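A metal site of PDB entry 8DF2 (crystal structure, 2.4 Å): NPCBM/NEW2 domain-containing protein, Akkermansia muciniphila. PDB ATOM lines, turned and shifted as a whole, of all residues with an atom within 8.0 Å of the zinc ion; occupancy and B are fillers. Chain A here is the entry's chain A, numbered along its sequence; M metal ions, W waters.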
ATOM      1  N   TYR A 171      23.435 -28.351  21.822  1.00  0.00           N
ATOM      2  CA  TYR A 171      22.853 -27.230  21.078  1.00  0.00           C
ATOM      3  C   TYR A 171      21.927 -26.503  22.044  1.00  0.00           C
ATOM      4  O   TYR A 171      20.779 -26.918  22.245  1.00  0.00           O
ATOM      5  CB  TYR A 171      22.088 -27.701  19.837  1.00  0.00           C
ATOM      6  CG  TYR A 171      22.912 -28.420  18.806  1.00  0.00           C
ATOM      7  CD1 TYR A 171      23.164 -29.789  18.913  1.00  0.00           C
ATOM      8  CD2 TYR A 171      23.431 -27.758  17.695  1.00  0.00           C
ATOM      9  CE1 TYR A 171      23.906 -30.473  17.964  1.00  0.00           C
ATOM     10  CE2 TYR A 171      24.174 -28.420  16.742  1.00  0.00           C
ATOM     11  CZ  TYR A 171      24.416 -29.779  16.877  1.00  0.00           C
ATOM     12  OH  TYR A 171      25.149 -30.458  15.927  1.00  0.00           O
ATOM     13  N   TYR A 172      22.427 -25.432  22.647  1.00  0.00           N
ATOM     14  CA  TYR A 172      21.695 -24.749  23.698  1.00  0.00           C
ATOM     15  C   TYR A 172      22.216 -23.327  23.790  1.00  0.00           C
ATOM     16  O   TYR A 172      23.362 -23.040  23.429  1.00  0.00           O
ATOM     17  CB  TYR A 172      21.860 -25.476  25.047  1.00  0.00           C
ATOM     18  CG  TYR A 172      21.114 -24.837  26.197  1.00  0.00           C
ATOM     19  CD1 TYR A 172      19.747 -25.045  26.384  1.00  0.00           C
ATOM     20  CD2 TYR A 172      21.785 -24.036  27.120  1.00  0.00           C
ATOM     21  CE1 TYR A 172      19.067 -24.458  27.434  1.00  0.00           C
ATOM     22  CE2 TYR A 172      21.104 -23.447  28.180  1.00  0.00           C
ATOM     23  CZ  TYR A 172      19.739 -23.662  28.327  1.00  0.00           C
ATOM     24  N   GLY A 173      21.339 -22.434  24.248  1.00  0.00           N
ATOM     25  CA  GLY A 173      21.706 -21.052  24.495  1.00  0.00           C
ATOM     26  C   GLY A 173      21.029 -20.559  25.756  1.00  0.00           C
ATOM     27  O   GLY A 173      19.855 -20.864  25.987  1.00  0.00           O
ATOM     28  N   GLY A 220      20.191 -22.168  14.000  1.00  0.00           N
ATOM     29  CA  GLY A 220      20.133 -22.548  15.400  1.00  0.00           C
ATOM     30  C   GLY A 220      21.129 -21.774  16.247  1.00  0.00           C
ATOM     31  O   GLY A 220      20.831 -21.369  17.374  1.00  0.00           O
ATOM     32  N   HIS A 223      19.802 -18.282  16.652  1.00  0.00           N
ATOM     33  CA  HIS A 223      18.693 -18.330  17.601  1.00  0.00           C
ATOM     34  C   HIS A 223      19.187 -18.533  19.027  1.00  0.00           C
ATOM     35  O   HIS A 223      18.819 -17.794  19.938  1.00  0.00           O
ATOM     36  CB  HIS A 223      17.747 -19.454  17.165  1.00  0.00           C
ATOM     37  CG  HIS A 223      16.658 -19.761  18.142  1.00  0.00           C
ATOM     38  ND1 HIS A 223      15.370 -19.313  17.977  1.00  0.00           N
ATOM     39  CD2 HIS A 223      16.652 -20.526  19.259  1.00  0.00           C
ATOM     40  CE1 HIS A 223      14.623 -19.767  18.971  1.00  0.00           C
ATOM     41  NE2 HIS A 223      15.376 -20.501  19.761  1.00  0.00           N
ATOM     42  N   GLU A 224      20.060 -19.531  19.239  1.00  0.00           N
ATOM     43  CA  GLU A 224      20.579 -19.798  20.567  1.00  0.00           C
ATOM     44  C   GLU A 224      21.456 -18.660  21.068  1.00  0.00           C
ATOM     45  O   GLU A 224      21.546 -18.428  22.280  1.00  0.00           O
ATOM     46  CB  GLU A 224      21.332 -21.118  20.589  1.00  0.00           C
ATOM     47  CG  GLU A 224      20.481 -22.263  21.097  1.00  0.00           C
ATOM     48  CD  GLU A 224      20.539 -23.487  20.204  1.00  0.00           C
ATOM     49  OE1 GLU A 224      21.632 -23.787  19.664  1.00  0.00           O
ATOM     50  OE2 GLU A 224      19.480 -24.146  20.056  1.00  0.00           O
ATOM     51  N   GLY A 226      20.679 -15.635  20.519  1.00  0.00           N
ATOM     52  CA  GLY A 226      19.661 -14.755  21.056  1.00  0.00           C
ATOM     53  C   GLY A 226      19.288 -15.098  22.490  1.00  0.00           C
ATOM     54  O   GLY A 226      19.100 -14.204  23.327  1.00  0.00           O
ATOM     55  N   HIS A 227      19.198 -16.399  22.797  1.00  0.00           N
ATOM     56  CA  HIS A 227      18.948 -16.805  24.175  1.00  0.00           C
ATOM     57  C   HIS A 227      20.065 -16.324  25.100  1.00  0.00           C
ATOM     58  O   HIS A 227      19.805 -15.852  26.206  1.00  0.00           O
ATOM     59  CB  HIS A 227      18.817 -18.327  24.267  1.00  0.00           C
ATOM     60  CG  HIS A 227      17.509 -18.852  23.771  1.00  0.00           C
ATOM     61  ND1 HIS A 227      16.308 -18.222  24.012  1.00  0.00           N
ATOM     62  CD2 HIS A 227      17.219 -19.965  23.040  1.00  0.00           C
ATOM     63  CE1 HIS A 227      15.335 -18.925  23.458  1.00  0.00           C
ATOM     64  NE2 HIS A 227      15.864 -19.975  22.865  1.00  0.00           N
ATOM     65  N   LEU A 231      17.098 -13.300  25.455  1.00  0.00           N
ATOM     66  CA  LEU A 231      15.803 -13.302  24.762  1.00  0.00           C
ATOM     67  C   LEU A 231      15.056 -14.613  25.019  1.00  0.00           C
ATOM     68  O   LEU A 231      15.648 -15.686  24.909  1.00  0.00           O
ATOM     69  CB  LEU A 231      15.991 -13.136  23.253  1.00  0.00           C
ATOM     70  CG  LEU A 231      16.648 -11.869  22.717  1.00  0.00           C
ATOM     71  CD1 LEU A 231      16.680 -11.922  21.181  1.00  0.00           C
ATOM     72  CD2 LEU A 231      15.921 -10.618  23.186  1.00  0.00           C
ATOM     73  N   PRO A 232      13.774 -14.554  25.362  1.00  0.00           N
ATOM     74  CA  PRO A 232      12.957 -15.776  25.376  1.00  0.00           C
ATOM     75  C   PRO A 232      12.474 -16.092  23.974  1.00  0.00           C
ATOM     76  O   PRO A 232      13.039 -15.620  22.980  1.00  0.00           O
ATOM     77  CB  PRO A 232      11.811 -15.417  26.310  1.00  0.00           C
ATOM     78  CG  PRO A 232      11.607 -13.974  26.039  1.00  0.00           C
ATOM     79  CD  PRO A 232      12.988 -13.380  25.803  1.00  0.00           C
ATOM     80  N   HIS A 233      11.420 -16.886  23.861  1.00  0.00           N
ATOM     81  CA  HIS A 233      10.840 -17.189  22.565  1.00  0.00           C
ATOM     82  C   HIS A 233       9.789 -16.150  22.228  1.00  0.00           C
ATOM     83  O   HIS A 233       9.040 -15.693  23.106  1.00  0.00           O
ATOM     84  CB  HIS A 233      10.232 -18.588  22.537  1.00  0.00           C
ATOM     85  CG  HIS A 233      11.244 -19.673  22.545  1.00  0.00           C
ATOM     86  ND1 HIS A 233      11.214 -20.711  23.457  1.00  0.00           N
ATOM     87  CD2 HIS A 233      12.352 -19.868  21.783  1.00  0.00           C
ATOM     88  CE1 HIS A 233      12.245 -21.509  23.240  1.00  0.00           C
ATOM     89  NE2 HIS A 233      12.944 -21.019  22.238  1.00  0.00           N
ATOM     90  N   THR A 234       9.762 -15.748  20.963  1.00  0.00           N
ATOM     91  CA  THR A 234       8.701 -14.909  20.429  1.00  0.00           C
ATOM     92  C   THR A 234       8.337 -15.467  19.064  1.00  0.00           C
ATOM     93  O   THR A 234       9.147 -15.403  18.133  1.00  0.00           O
ATOM     94  CB  THR A 234       9.114 -13.438  20.325  1.00  0.00           C
ATOM     95  OG1 THR A 234       9.398 -12.916  21.632  1.00  0.00           O
ATOM     96  CG2 THR A 234       7.998 -12.620  19.691  1.00  0.00           C
ATOM     97  N   LEU A 247      12.891 -14.875  14.305  1.00  0.00           N
ATOM     98  CA  LEU A 247      14.109 -15.619  14.613  1.00  0.00           C
ATOM     99  C   LEU A 247      13.984 -16.366  15.936  1.00  0.00           C
ATOM    100  O   LEU A 247      14.321 -17.555  16.023  1.00  0.00           O
ATOM    101  CB  LEU A 247      15.303 -14.657  14.670  1.00  0.00           C
ATOM    102  CG  LEU A 247      16.606 -15.222  15.223  1.00  0.00           C
ATOM    103  CD1 LEU A 247      17.360 -15.980  14.146  1.00  0.00           C
ATOM    104  CD2 LEU A 247      17.476 -14.112  15.750  1.00  0.00           C
ATOM    105  N   MET A 248      13.490 -15.688  16.965  1.00  0.00           N
ATOM    106  CA  MET A 248      13.341 -16.285  18.280  1.00  0.00           C
ATOM    107  C   MET A 248      12.075 -17.142  18.416  1.00  0.00           C
ATOM    108  O   MET A 248      11.709 -17.505  19.539  1.00  0.00           O
ATOM    109  CB  MET A 248      13.372 -15.196  19.343  1.00  0.00           C
ATOM    110  CG  MET A 248      14.758 -14.539  19.502  1.00  0.00           C
ATOM    111  SD  MET A 248      16.170 -15.676  19.452  1.00  0.00           S
ATOM    112  CE  MET A 248      15.798 -16.723  20.863  1.00  0.00           C
ATOM    113  N   GLY A 249      11.380 -17.420  17.315  1.00  0.00           N
ATOM    114  CA  GLY A 249      10.300 -18.384  17.334  1.00  0.00           C
ATOM    115  C   GLY A 249      10.787 -19.703  16.778  1.00  0.00           C
ATOM    116  O   GLY A 249      11.450 -20.485  17.473  1.00  0.00           O
ATOM    117  N   HIS A 250      10.470 -19.973  15.505  1.00  0.00           N
ATOM    118  CA  HIS A 250      11.043 -21.098  14.805  1.00  0.00           C
ATOM    119  C   HIS A 250      11.861 -20.650  13.590  1.00  0.00           C
ATOM    120  O   HIS A 250      12.134 -21.442  12.676  1.00  0.00           O
ATOM    121  CB  HIS A 250       9.954 -22.114  14.416  1.00  0.00           C
ATOM    122  CG  HIS A 250       9.008 -21.617  13.368  1.00  0.00           C
ATOM    123  ND1 HIS A 250       9.410 -21.287  12.090  1.00  0.00           N
ATOM    124  CD2 HIS A 250       7.668 -21.417  13.399  1.00  0.00           C
ATOM    125  CE1 HIS A 250       8.374 -20.902  11.385  1.00  0.00           C
ATOM    126  NE2 HIS A 250       7.301 -20.966  12.155  1.00  0.00           N
ATOM    127  N   ASN A 252      14.888 -20.249  13.525  1.00  0.00           N
ATOM    128  CA  ASN A 252      16.113 -21.020  13.411  1.00  0.00           C
ATOM    129  C   ASN A 252      16.073 -22.016  12.260  1.00  0.00           C
ATOM    130  O   ASN A 252      17.123 -22.392  11.743  1.00  0.00           O
ATOM    131  CB  ASN A 252      16.400 -21.762  14.716  1.00  0.00           C
ATOM    132  CG  ASN A 252      15.194 -22.493  15.248  1.00  0.00           C
ATOM    133  OD1 ASN A 252      14.138 -21.909  15.411  1.00  0.00           O
ATOM    134  ND2 ASN A 252      15.351 -23.785  15.521  1.00  0.00           N
ATOM    135  N   LEU A 299      13.918 -16.015  30.456  1.00  0.00           N
ATOM    136  CA  LEU A 299      15.312 -15.624  30.359  1.00  0.00           C
ATOM    137  C   LEU A 299      15.463 -14.119  30.577  1.00  0.00           C
ATOM    138  O   LEU A 299      14.547 -13.344  30.333  1.00  0.00           O
ATOM    139  CB  LEU A 299      15.886 -16.032  28.999  1.00  0.00           C
ATOM    140  CG  LEU A 299      16.231 -17.508  28.833  1.00  0.00           C
ATOM    141  CD1 LEU A 299      16.770 -17.779  27.425  1.00  0.00           C
ATOM    142  CD2 LEU A 299      17.254 -17.940  29.902  1.00  0.00           C
ATOM    143  N   SER A 344       4.753 -24.465  25.092  1.00  0.00           N
ATOM    144  CA  SER A 344       5.782 -23.539  25.577  1.00  0.00           C
ATOM    145  C   SER A 344       5.488 -22.133  25.065  1.00  0.00           C
ATOM    146  O   SER A 344       4.337 -21.804  24.763  1.00  0.00           O
ATOM    147  CB  SER A 344       7.181 -24.008  25.149  1.00  0.00           C
ATOM    148  OG  SER A 344       8.159 -23.047  25.473  1.00  0.00           O
ATOM    149  N   ASP A 345       6.511 -21.278  24.962  1.00  0.00           N
ATOM    150  CA  ASP A 345       6.305 -19.920  24.452  1.00  0.00           C
ATOM    151  C   ASP A 345       6.608 -19.790  22.963  1.00  0.00           C
ATOM    152  O   ASP A 345       6.688 -18.666  22.455  1.00  0.00           O
ATOM    153  CB  ASP A 345       7.145 -18.907  25.261  1.00  0.00           C
ATOM    154  CG  ASP A 345       8.625 -19.285  25.368  1.00  0.00           C
ATOM    155  OD1 ASP A 345       8.980 -20.446  25.064  1.00  0.00           O
ATOM    156  OD2 ASP A 345       9.429 -18.406  25.742  1.00  0.00           O
ATOM    157  N   TYR A 346       6.737 -20.918  22.259  1.00  0.00           N
ATOM    158  CA  TYR A 346       6.996 -20.883  20.817  1.00  0.00           C
ATOM    159  C   TYR A 346       5.827 -20.262  20.064  1.00  0.00           C
ATOM    160  O   TYR A 346       6.020 -19.569  19.058  1.00  0.00           O
ATOM    161  CB  TYR A 346       7.266 -22.285  20.299  1.00  0.00           C
ATOM    162  CG  TYR A 346       8.591 -22.864  20.703  1.00  0.00           C
ATOM    163  CD1 TYR A 346       9.779 -22.335  20.208  1.00  0.00           C
ATOM    164  CD2 TYR A 346       8.656 -23.950  21.566  1.00  0.00           C
ATOM    165  CE1 TYR A 346      11.000 -22.864  20.569  1.00  0.00           C
ATOM    166  CE2 TYR A 346       9.872 -24.488  21.928  1.00  0.00           C
ATOM    167  CZ  TYR A 346      11.042 -23.950  21.431  1.00  0.00           C
ATOM    168  OH  TYR A 346      12.263 -24.479  21.792  1.00  0.00           O
HETATM  169 ZN    ZN M   1      15.015 -21.713  21.670  1.00  0.00          ZN
HETATM  170  O   HOH W   1      16.905 -23.462  21.697  1.00  0.00           O
HETATM  171  O   HOH W   2      15.286 -23.421  23.264  1.00  0.00           O
HETATM  172  O   HOH W   3      14.245 -23.760  20.108  1.00  0.00           O
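A ring nitrogen (ND1) of His 233 is in hydrogen-bond range of the side-chain carboxylate (OD1) of Asp 345. ND1 of His 227 lies within hydrogen-bond range of O of Leu 231, 2.8 Å away. A ring nitrogen (ND1) of His 223 sits at hydrogen-bond distance from the backbone carbonyl oxygen (O) of Leu 247, 2.8 Å away.
OH of Tyr 346 touches the zinc ion, at 3.9 Å. The nearest printed residue that does not touch the zinc ion is Met 248 (5.1 Å).
A ring nitrogen (NE2) of His 233 binds the zinc ion. A ring nitrogen (NE2) of His 227 is bound to the zinc ion (2.3 Å). NE2 of His 223 is bound to the zinc ion, 2.3 Å away. Water W2 is bound to the zinc ion (2.4 Å). Water W1 binds the zinc ion, 2.6 Å away. Slightly farther from the zinc ion lies water W3 (2.7 Å).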
